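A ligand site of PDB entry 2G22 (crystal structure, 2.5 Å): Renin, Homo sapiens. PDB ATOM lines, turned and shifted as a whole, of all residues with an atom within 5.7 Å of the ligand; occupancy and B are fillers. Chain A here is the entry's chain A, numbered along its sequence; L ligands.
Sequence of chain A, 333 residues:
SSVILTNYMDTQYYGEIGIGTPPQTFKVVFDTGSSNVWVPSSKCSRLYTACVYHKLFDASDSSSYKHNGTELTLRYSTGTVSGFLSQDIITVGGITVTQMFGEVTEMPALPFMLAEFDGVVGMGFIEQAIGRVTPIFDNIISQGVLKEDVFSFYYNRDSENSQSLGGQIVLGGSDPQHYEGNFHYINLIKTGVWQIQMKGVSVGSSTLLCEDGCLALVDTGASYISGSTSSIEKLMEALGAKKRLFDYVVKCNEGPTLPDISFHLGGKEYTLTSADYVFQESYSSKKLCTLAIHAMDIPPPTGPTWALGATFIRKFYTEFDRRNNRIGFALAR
Thr 11 touches the ligand. NE2 of Gln 12 touches C15 of the ligand (3.6 Å). Val 29 touches the ligand (CB to C6, 3.7 Å). CA of Gly 33 touches N4 of the ligand (3.7 Å). Tyr 76 touches the ligand. Pro 111 touches the ligand. Phe 112 touches the ligand (CE2 to C8, 3.8 Å). Ala 115 touches the ligand. CE1 of Phe 117 touches C14 of the ligand, at 3.7 Å. CG2 of Val 120 touches C5 of the ligand, 3.7 Å away. Thr 220 touches the ligand (O to C19, 3.4 Å). Gly 221 touches the ligand (O to C18, 3.2 Å). CB of Ala 222 touches C21 of the ligand, at 3.8 Å. Ser 223 touches the ligand. Tyr 224 touches the ligand. SD of Met 296 touches C24 of the ligand, at 3.4 Å. Within 4 Å of the ligand: Thr 11, Gln 12, Tyr 13, Val 29, Asp 31, Gly 33, Tyr 76, Thr 78, Pro 111, Phe 112, Ala 115, Phe 117, Val 120, Asp 219, Thr 220, Gly 221, Ala 222, Ser 223, Tyr 224 and Met 296. The nearest printed residue that does not touch the ligand is Ser 77 (4.01 Å).
The side-chain carboxylate (OD1) of Asp 31 sits at hydrogen-bond distance from a nitrogen (N2) of the ligand. N4 of the ligand lies within hydrogen-bond range of OD1 of Asp 219 (3.2 Å). N3 of the ligand lies within hydrogen-bond range of OG1 of Thr 78 (3.2 Å). The backbone NH (N) of Tyr 13 is in hydrogen-bond range of an oxygen (O1) of the ligand.
The side-chain carboxylate of Asp 31 lies close to the backbone NH of Gly 221, at 3.4 Å. OD2 of Asp 31 is in hydrogen-bond range of N of Gly 33 (2.4 Å). The side-chain carboxylate of Asp 31 lies within hydrogen-bond range of the side-chain hydroxyl of Ser 34. OD2 of Asp 219 is in hydrogen-bond range of N of Gly 33. OD2 of Asp 219 is in hydrogen-bond range of N of Ala 222, 3.5 Å away. The backbone carbonyl oxygen (O) of Thr 11 sits at hydrogen-bond distance from the side-chain hydroxyl (OG) of Ser 223 (2.4 Å). The side-chain amide oxygen of Gln 12 is in hydrogen-bond range of the backbone NH of Glu 116. N of Ala 310 sits at hydrogen-bond distance from O of Ala 222.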
ATOM      1  N   THR A  11      14.943  -1.598  25.773  1.00  0.00           N
ATOM      2  CA  THR A  11      16.035  -0.654  25.542  1.00  0.00           C
ATOM      3  C   THR A  11      15.928   0.080  24.217  1.00  0.00           C
ATOM      4  O   THR A  11      16.630   1.067  23.995  1.00  0.00           O
ATOM      5  CB  THR A  11      17.415  -1.352  25.605  1.00  0.00           C
ATOM      6  OG1 THR A  11      17.484  -2.416  24.636  1.00  0.00           O
ATOM      7  CG2 THR A  11      17.661  -1.922  26.983  1.00  0.00           C
ATOM      8  N   GLN A  12      15.043  -0.397  23.344  1.00  0.00           N
ATOM      9  CA  GLN A  12      14.847   0.248  22.045  1.00  0.00           C
ATOM     10  C   GLN A  12      13.373   0.310  21.675  1.00  0.00           C
ATOM     11  O   GLN A  12      12.670  -0.709  21.718  1.00  0.00           O
ATOM     12  CB  GLN A  12      15.620  -0.510  20.964  1.00  0.00           C
ATOM     13  CG  GLN A  12      17.132  -0.365  21.072  1.00  0.00           C
ATOM     14  CD  GLN A  12      17.882  -1.275  20.112  1.00  0.00           C
ATOM     15  OE1 GLN A  12      17.570  -1.331  18.925  1.00  0.00           O
ATOM     16  NE2 GLN A  12      18.869  -1.987  20.626  1.00  0.00           N
ATOM     17  N   TYR A  13      12.903   1.502  21.336  1.00  0.00           N
ATOM     18  CA  TYR A  13      11.517   1.708  20.930  1.00  0.00           C
ATOM     19  C   TYR A  13      11.539   2.342  19.542  1.00  0.00           C
ATOM     20  O   TYR A  13      12.117   3.419  19.353  1.00  0.00           O
ATOM     21  CB  TYR A  13      10.781   2.631  21.907  1.00  0.00           C
ATOM     22  CG  TYR A  13      10.531   2.040  23.275  1.00  0.00           C
ATOM     23  CD1 TYR A  13      11.480   2.126  24.272  1.00  0.00           C
ATOM     24  CD2 TYR A  13       9.332   1.380  23.562  1.00  0.00           C
ATOM     25  CE1 TYR A  13      11.255   1.576  25.526  1.00  0.00           C
ATOM     26  CE2 TYR A  13       9.102   0.836  24.809  1.00  0.00           C
ATOM     27  CZ  TYR A  13      10.058   0.935  25.780  1.00  0.00           C
ATOM     28  OH  TYR A  13       9.838   0.382  27.026  1.00  0.00           O
ATOM     29  N   VAL A  29      13.687   5.346  15.316  1.00  0.00           N
ATOM     30  CA  VAL A  29      13.441   5.788  16.680  1.00  0.00           C
ATOM     31  C   VAL A  29      13.041   7.280  16.689  1.00  0.00           C
ATOM     32  O   VAL A  29      13.753   8.121  16.150  1.00  0.00           O
ATOM     33  CB  VAL A  29      14.687   5.659  17.585  1.00  0.00           C
ATOM     34  CG1 VAL A  29      14.365   6.148  18.980  1.00  0.00           C
ATOM     35  CG2 VAL A  29      15.140   4.215  17.643  1.00  0.00           C
ATOM     36  N   ASP A  31      13.177  10.356  18.267  1.00  0.00           N
ATOM     37  CA  ASP A  31      14.121  10.897  19.233  1.00  0.00           C
ATOM     38  C   ASP A  31      14.039  12.387  19.536  1.00  0.00           C
ATOM     39  O   ASP A  31      14.348  13.200  18.682  1.00  0.00           O
ATOM     40  CB  ASP A  31      15.511  10.552  18.688  1.00  0.00           C
ATOM     41  CG  ASP A  31      16.638  11.157  19.471  1.00  0.00           C
ATOM     42  OD1 ASP A  31      17.740  11.272  18.903  1.00  0.00           O
ATOM     43  OD2 ASP A  31      16.413  11.497  20.649  1.00  0.00           O
ATOM     44  N   GLY A  33      15.948  13.747  21.458  1.00  0.00           N
ATOM     45  CA  GLY A  33      17.307  14.151  21.754  1.00  0.00           C
ATOM     46  C   GLY A  33      18.108  14.590  20.543  1.00  0.00           C
ATOM     47  O   GLY A  33      19.286  14.941  20.685  1.00  0.00           O
ATOM     48  N   SER A  34      17.504  14.561  19.362  1.00  0.00           N
ATOM     49  CA  SER A  34      18.183  15.001  18.145  1.00  0.00           C
ATOM     50  C   SER A  34      17.170  15.704  17.247  1.00  0.00           C
ATOM     51  O   SER A  34      15.979  15.685  17.525  1.00  0.00           O
ATOM     52  CB  SER A  34      18.835  13.806  17.424  1.00  0.00           C
ATOM     53  OG  SER A  34      17.866  12.901  16.920  1.00  0.00           O
ATOM     54  N   TYR A  76      25.965  11.195  18.460  1.00  0.00           N
ATOM     55  CA  TYR A  76      25.153  10.894  19.633  1.00  0.00           C
ATOM     56  C   TYR A  76      26.199  10.574  20.694  1.00  0.00           C
ATOM     57  O   TYR A  76      27.369  10.378  20.373  1.00  0.00           O
ATOM     58  CB  TYR A  76      24.243   9.703  19.360  1.00  0.00           C
ATOM     59  CG  TYR A  76      23.318   9.914  18.184  1.00  0.00           C
ATOM     60  CD1 TYR A  76      23.619   9.415  16.931  1.00  0.00           C
ATOM     61  CD2 TYR A  76      22.136  10.638  18.335  1.00  0.00           C
ATOM     62  CE1 TYR A  76      22.784   9.635  15.850  1.00  0.00           C
ATOM     63  CE2 TYR A  76      21.297  10.872  17.272  1.00  0.00           C
ATOM     64  CZ  TYR A  76      21.620  10.365  16.025  1.00  0.00           C
ATOM     65  OH  TYR A  76      20.787  10.594  14.967  1.00  0.00           O
ATOM     66  N   SER A  77      25.776  10.507  21.949  1.00  0.00           N
ATOM     67  CA  SER A  77      26.721  10.230  23.026  1.00  0.00           C
ATOM     68  C   SER A  77      27.344   8.836  22.965  1.00  0.00           C
ATOM     69  O   SER A  77      28.359   8.588  23.593  1.00  0.00           O
ATOM     70  CB  SER A  77      26.034  10.429  24.378  1.00  0.00           C
ATOM     71  OG  SER A  77      25.539  11.755  24.490  1.00  0.00           O
ATOM     72  N   THR A  78      26.748   7.954  22.184  1.00  0.00           N
ATOM     73  CA  THR A  78      27.228   6.581  22.105  1.00  0.00           C
ATOM     74  C   THR A  78      27.646   6.114  20.714  1.00  0.00           C
ATOM     75  O   THR A  78      27.968   4.942  20.524  1.00  0.00           O
ATOM     76  CB  THR A  78      26.144   5.613  22.619  1.00  0.00           C
ATOM     77  OG1 THR A  78      24.915   5.874  21.929  1.00  0.00           O
ATOM     78  CG2 THR A  78      25.933   5.786  24.103  1.00  0.00           C
ATOM     79  N   GLY A  79      27.643   7.022  19.748  1.00  0.00           N
ATOM     80  CA  GLY A  79      28.017   6.637  18.410  1.00  0.00           C
ATOM     81  C   GLY A  79      27.814   7.719  17.378  1.00  0.00           C
ATOM     82  O   GLY A  79      27.097   8.689  17.622  1.00  0.00           O
ATOM     83  N   PRO A 111      28.004   1.096  17.726  1.00  0.00           N
ATOM     84  CA  PRO A 111      26.965   0.182  18.186  1.00  0.00           C
ATOM     85  C   PRO A 111      25.875  -0.243  17.215  1.00  0.00           C
ATOM     86  O   PRO A 111      25.030  -1.044  17.596  1.00  0.00           O
ATOM     87  CB  PRO A 111      26.340   0.964  19.308  1.00  0.00           C
ATOM     88  CG  PRO A 111      26.197   2.318  18.604  1.00  0.00           C
ATOM     89  CD  PRO A 111      27.569   2.486  17.930  1.00  0.00           C
ATOM     90  N   PHE A 112      25.868   0.250  15.979  1.00  0.00           N
ATOM     91  CA  PHE A 112      24.738  -0.061  15.088  1.00  0.00           C
ATOM     92  C   PHE A 112      24.401  -1.490  14.703  1.00  0.00           C
ATOM     93  O   PHE A 112      23.294  -1.755  14.218  1.00  0.00           O
ATOM     94  CB  PHE A 112      24.779   0.870  13.875  1.00  0.00           C
ATOM     95  CG  PHE A 112      24.712   2.316  14.271  1.00  0.00           C
ATOM     96  CD1 PHE A 112      25.858   3.084  14.351  1.00  0.00           C
ATOM     97  CD2 PHE A 112      23.530   2.856  14.739  1.00  0.00           C
ATOM     98  CE1 PHE A 112      25.824   4.348  14.906  1.00  0.00           C
ATOM     99  CE2 PHE A 112      23.490   4.126  15.287  1.00  0.00           C
ATOM    100  CZ  PHE A 112      24.639   4.861  15.383  1.00  0.00           C
ATOM    101  N   LEU A 114      24.070  -3.557  16.887  1.00  0.00           N
ATOM    102  CA  LEU A 114      23.203  -3.869  18.015  1.00  0.00           C
ATOM    103  C   LEU A 114      21.903  -3.111  17.907  1.00  0.00           C
ATOM    104  O   LEU A 114      21.054  -3.190  18.800  1.00  0.00           O
ATOM    105  CB  LEU A 114      23.888  -3.508  19.334  1.00  0.00           C
ATOM    106  CG  LEU A 114      25.266  -4.092  19.643  1.00  0.00           C
ATOM    107  CD1 LEU A 114      25.676  -3.652  21.035  1.00  0.00           C
ATOM    108  CD2 LEU A 114      25.251  -5.604  19.537  1.00  0.00           C
ATOM    109  N   ALA A 115      21.726  -2.364  16.823  1.00  0.00           N
ATOM    110  CA  ALA A 115      20.500  -1.599  16.622  1.00  0.00           C
ATOM    111  C   ALA A 115      19.443  -2.409  15.891  1.00  0.00           C
ATOM    112  O   ALA A 115      19.695  -2.969  14.821  1.00  0.00           O
ATOM    113  CB  ALA A 115      20.800  -0.337  15.849  1.00  0.00           C
ATOM    114  N   GLU A 116      18.254  -2.465  16.479  1.00  0.00           N
ATOM    115  CA  GLU A 116      17.144  -3.172  15.863  1.00  0.00           C
ATOM    116  C   GLU A 116      16.509  -2.248  14.828  1.00  0.00           C
ATOM    117  O   GLU A 116      15.897  -2.704  13.865  1.00  0.00           O
ATOM    118  CB  GLU A 116      16.097  -3.539  16.915  1.00  0.00           C
ATOM    119  CG  GLU A 116      16.073  -5.004  17.294  1.00  0.00           C
ATOM    120  CD  GLU A 116      15.655  -5.888  16.137  1.00  0.00           C
ATOM    121  OE1 GLU A 116      14.663  -5.569  15.458  1.00  0.00           O
ATOM    122  OE2 GLU A 116      16.332  -6.922  15.917  1.00  0.00           O
ATOM    123  N   PHE A 117      16.646  -0.944  15.037  1.00  0.00           N
ATOM    124  CA  PHE A 117      16.092   0.023  14.105  1.00  0.00           C
ATOM    125  C   PHE A 117      17.086   0.271  13.001  1.00  0.00           C
ATOM    126  O   PHE A 117      18.237  -0.153  13.103  1.00  0.00           O
ATOM    127  CB  PHE A 117      15.772   1.361  14.804  1.00  0.00           C
ATOM    128  CG  PHE A 117      16.911   1.906  15.633  1.00  0.00           C
ATOM    129  CD1 PHE A 117      17.124   1.446  16.933  1.00  0.00           C
ATOM    130  CD2 PHE A 117      17.753   2.893  15.137  1.00  0.00           C
ATOM    131  CE1 PHE A 117      18.155   1.961  17.713  1.00  0.00           C
ATOM    132  CE2 PHE A 117      18.784   3.407  15.917  1.00  0.00           C
ATOM    133  CZ  PHE A 117      18.979   2.939  17.208  1.00  0.00           C
ATOM    134  N   VAL A 120      16.813   7.124  12.338  1.00  0.00           N
ATOM    135  CA  VAL A 120      16.257   7.989  13.347  1.00  0.00           C
ATOM    136  C   VAL A 120      15.450   9.154  12.800  1.00  0.00           C
ATOM    137  O   VAL A 120      15.703   9.660  11.711  1.00  0.00           O
ATOM    138  CB  VAL A 120      17.390   8.582  14.229  1.00  0.00           C
ATOM    139  CG1 VAL A 120      16.797   9.463  15.320  1.00  0.00           C
ATOM    140  CG2 VAL A 120      18.241   7.450  14.818  1.00  0.00           C
ATOM    141  N   TYR A 155       5.700   4.588  26.415  1.00  0.00           N
ATOM    142  CA  TYR A 155       6.613   3.449  26.296  1.00  0.00           C
ATOM    143  C   TYR A 155       6.117   2.411  27.279  1.00  0.00           C
ATOM    144  O   TYR A 155       6.187   2.604  28.500  1.00  0.00           O
ATOM    145  CB  TYR A 155       8.036   3.835  26.668  1.00  0.00           C
ATOM    146  CG  TYR A 155       8.829   4.537  25.589  1.00  0.00           C
ATOM    147  CD1 TYR A 155      10.073   5.072  25.868  1.00  0.00           C
ATOM    148  CD2 TYR A 155       8.338   4.684  24.314  1.00  0.00           C
ATOM    149  CE1 TYR A 155      10.806   5.723  24.909  1.00  0.00           C
ATOM    150  CE2 TYR A 155       9.058   5.333  23.347  1.00  0.00           C
ATOM    151  CZ  TYR A 155      10.296   5.855  23.652  1.00  0.00           C
ATOM    152  OH  TYR A 155      11.036   6.524  22.704  1.00  0.00           O
ATOM    153  N   ASP A 219      15.062  12.845  26.931  1.00  0.00           N
ATOM    154  CA  ASP A 219      15.437  12.140  25.709  1.00  0.00           C
ATOM    155  C   ASP A 219      14.673  10.844  25.386  1.00  0.00           C
ATOM    156  O   ASP A 219      14.950   9.787  25.962  1.00  0.00           O
ATOM    157  CB  ASP A 219      16.950  11.856  25.811  1.00  0.00           C
ATOM    158  CG  ASP A 219      17.587  11.562  24.476  1.00  0.00           C
ATOM    159  OD1 ASP A 219      18.838  11.551  24.430  1.00  0.00           O
ATOM    160  OD2 ASP A 219      16.864  11.345  23.481  1.00  0.00           O
ATOM    161  N   THR A 220      13.740  10.923  24.436  1.00  0.00           N
ATOM    162  CA  THR A 220      12.973   9.737  24.042  1.00  0.00           C
ATOM    163  C   THR A 220      13.866   8.775  23.252  1.00  0.00           C
ATOM    164  O   THR A 220      13.499   7.622  23.029  1.00  0.00           O
ATOM    165  CB  THR A 220      11.741  10.080  23.151  1.00  0.00           C
ATOM    166  OG1 THR A 220      12.176  10.754  21.966  1.00  0.00           O
ATOM    167  CG2 THR A 220      10.752  10.954  23.924  1.00  0.00           C
ATOM    168  N   GLY A 221      15.034   9.259  22.836  1.00  0.00           N
ATOM    169  CA  GLY A 221      15.945   8.424  22.071  1.00  0.00           C
ATOM    170  C   GLY A 221      16.988   7.740  22.944  1.00  0.00           C
ATOM    171  O   GLY A 221      17.857   7.025  22.434  1.00  0.00           O
ATOM    172  N   ALA A 222      16.905   7.955  24.256  1.00  0.00           N
ATOM    173  CA  ALA A 222      17.842   7.363  25.197  1.00  0.00           C
ATOM    174  C   ALA A 222      17.243   6.191  25.959  1.00  0.00           C
ATOM    175  O   ALA A 222      16.149   6.285  26.526  1.00  0.00           O
ATOM    176  CB  ALA A 222      18.331   8.434  26.175  1.00  0.00           C
ATOM    177  N   SER A 223      17.976   5.084  25.998  1.00  0.00           N
ATOM    178  CA  SER A 223      17.529   3.884  26.697  1.00  0.00           C
ATOM    179  C   SER A 223      17.380   4.037  28.206  1.00  0.00           C
ATOM    180  O   SER A 223      16.522   3.419  28.811  1.00  0.00           O
ATOM    181  CB  SER A 223      18.490   2.730  26.438  1.00  0.00           C
ATOM    182  OG  SER A 223      18.435   2.292  25.097  1.00  0.00           O
ATOM    183  N   TYR A 224      18.201   4.878  28.812  1.00  0.00           N
ATOM    184  CA  TYR A 224      18.163   4.987  30.262  1.00  0.00           C
ATOM    185  C   TYR A 224      17.996   6.373  30.855  1.00  0.00           C
ATOM    186  O   TYR A 224      17.685   7.346  30.176  1.00  0.00           O
ATOM    187  CB  TYR A 224      19.456   4.375  30.817  1.00  0.00           C
ATOM    188  CG  TYR A 224      19.856   3.082  30.142  1.00  0.00           C
ATOM    189  CD1 TYR A 224      21.012   3.003  29.369  1.00  0.00           C
ATOM    190  CD2 TYR A 224      19.045   1.947  30.233  1.00  0.00           C
ATOM    191  CE1 TYR A 224      21.353   1.812  28.713  1.00  0.00           C
ATOM    192  CE2 TYR A 224      19.370   0.768  29.588  1.00  0.00           C
ATOM    193  CZ  TYR A 224      20.526   0.700  28.824  1.00  0.00           C
ATOM    194  OH  TYR A 224      20.804  -0.477  28.171  1.00  0.00           O
ATOM    195  N   HIS A 294      22.400   4.902  33.985  1.00  0.00           N
ATOM    196  CA  HIS A 294      23.817   4.933  33.602  1.00  0.00           C
ATOM    197  C   HIS A 294      24.486   6.281  33.812  1.00  0.00           C
ATOM    198  O   HIS A 294      23.830   7.291  34.057  1.00  0.00           O
ATOM    199  CB  HIS A 294      23.991   4.549  32.127  1.00  0.00           C
ATOM    200  CG  HIS A 294      23.770   3.105  31.839  1.00  0.00           C
ATOM    201  ND1 HIS A 294      24.621   2.370  31.044  1.00  0.00           N
ATOM    202  CD2 HIS A 294      22.787   2.247  32.239  1.00  0.00           C
ATOM    203  CE1 HIS A 294      24.173   1.127  30.955  1.00  0.00           C
ATOM    204  NE2 HIS A 294      23.063   1.030  31.665  1.00  0.00           N
ATOM    205  N   MET A 296      26.747   9.167  32.122  1.00  0.00           N
ATOM    206  CA  MET A 296      27.022   9.650  30.776  1.00  0.00           C
ATOM    207  C   MET A 296      27.265  11.141  30.792  1.00  0.00           C
ATOM    208  O   MET A 296      26.350  11.934  30.971  1.00  0.00           O
ATOM    209  CB  MET A 296      25.840   9.349  29.859  1.00  0.00           C
ATOM    210  CG  MET A 296      26.094   9.696  28.414  1.00  0.00           C
ATOM    211  SD  MET A 296      25.229   8.523  27.373  1.00  0.00           S
ATOM    212  CE  MET A 296      25.961   6.975  28.009  1.00  0.00           C
ATOM    213  N   ALA A 310      14.082   6.204  28.335  1.00  0.00           N
ATOM    214  CA  ALA A 310      13.065   5.169  28.425  1.00  0.00           C
ATOM    215  C   ALA A 310      12.712   4.710  29.848  1.00  0.00           C
ATOM    216  O   ALA A 310      11.548   4.471  30.168  1.00  0.00           O
ATOM    217  CB  ALA A 310      13.488   3.969  27.587  1.00  0.00           C
HETATM  218  C1  LIG L   1      21.341   8.185  21.532  1.00  0.00           C
HETATM  219  N1  LIG L   1      20.901   9.434  21.853  1.00  0.00           N
HETATM  220  C2  LIG L   1      20.016   9.996  21.035  1.00  0.00           C
HETATM  221  N2  LIG L   1      19.542   9.435  19.928  1.00  0.00           N
HETATM  222  C3  LIG L   1      19.965   8.192  19.580  1.00  0.00           C
HETATM  223  C4  LIG L   1      20.900   7.480  20.389  1.00  0.00           C
HETATM  224  N3  LIG L   1      22.253   7.652  22.420  1.00  0.00           N
HETATM  225  N4  LIG L   1      19.579  11.211  21.384  1.00  0.00           N
HETATM  226  C5  LIG L   1      19.352   7.652  18.304  1.00  0.00           C
HETATM  227  C6  LIG L   1      17.964   7.088  18.538  1.00  0.00           C
HETATM  228  C7  LIG L   1      22.473   5.791  19.245  1.00  0.00           C
HETATM  229  C8  LIG L   1      22.818   4.437  18.990  1.00  0.00           C
HETATM  230  C9  LIG L   1      22.066   3.358  19.547  1.00  0.00           C
HETATM  231  C10 LIG L   1      20.944   3.651  20.384  1.00  0.00           C
HETATM  232  C11 LIG L   1      20.640   5.015  20.613  1.00  0.00           C
HETATM  233  C12 LIG L   1      21.368   6.086  20.069  1.00  0.00           C
HETATM  234  C13 LIG L   1      22.484   1.922  19.247  1.00  0.00           C
HETATM  235  C14 LIG L   1      21.321   0.918  19.415  1.00  0.00           C
HETATM  236  C15 LIG L   1      20.505   1.172  20.720  1.00  0.00           C
HETATM  237  N5  LIG L   1      20.172   2.598  20.968  1.00  0.00           N
HETATM  238  C16 LIG L   1      19.049   2.859  21.907  1.00  0.00           C
HETATM  239  C17 LIG L   1      17.701   3.219  21.237  1.00  0.00           C
HETATM  240  C18 LIG L   1      16.798   3.977  22.217  1.00  0.00           C
HETATM  241  O1  LIG L   1      15.433   3.767  21.916  1.00  0.00           O
HETATM  242  C19 LIG L   1      14.537   4.434  22.784  1.00  0.00           C
HETATM  243  C20 LIG L   1      22.649   8.427  23.605  1.00  0.00           C
HETATM  244  C21 LIG L   1      21.902   7.999  24.861  1.00  0.00           C
HETATM  245  C22 LIG L   1      22.474   3.816  25.997  1.00  0.00           C
HETATM  246  C23 LIG L   1      23.164   4.865  26.674  1.00  0.00           C
HETATM  247  C24 LIG L   1      22.958   6.212  26.286  1.00  0.00           C
HETATM  248  C25 LIG L   1      22.070   6.542  25.228  1.00  0.00           C
HETATM  249  C26 LIG L   1      21.383   5.477  24.547  1.00  0.00           C
HETATM  250  C27 LIG L   1      21.584   4.122  24.934  1.00  0.00           C
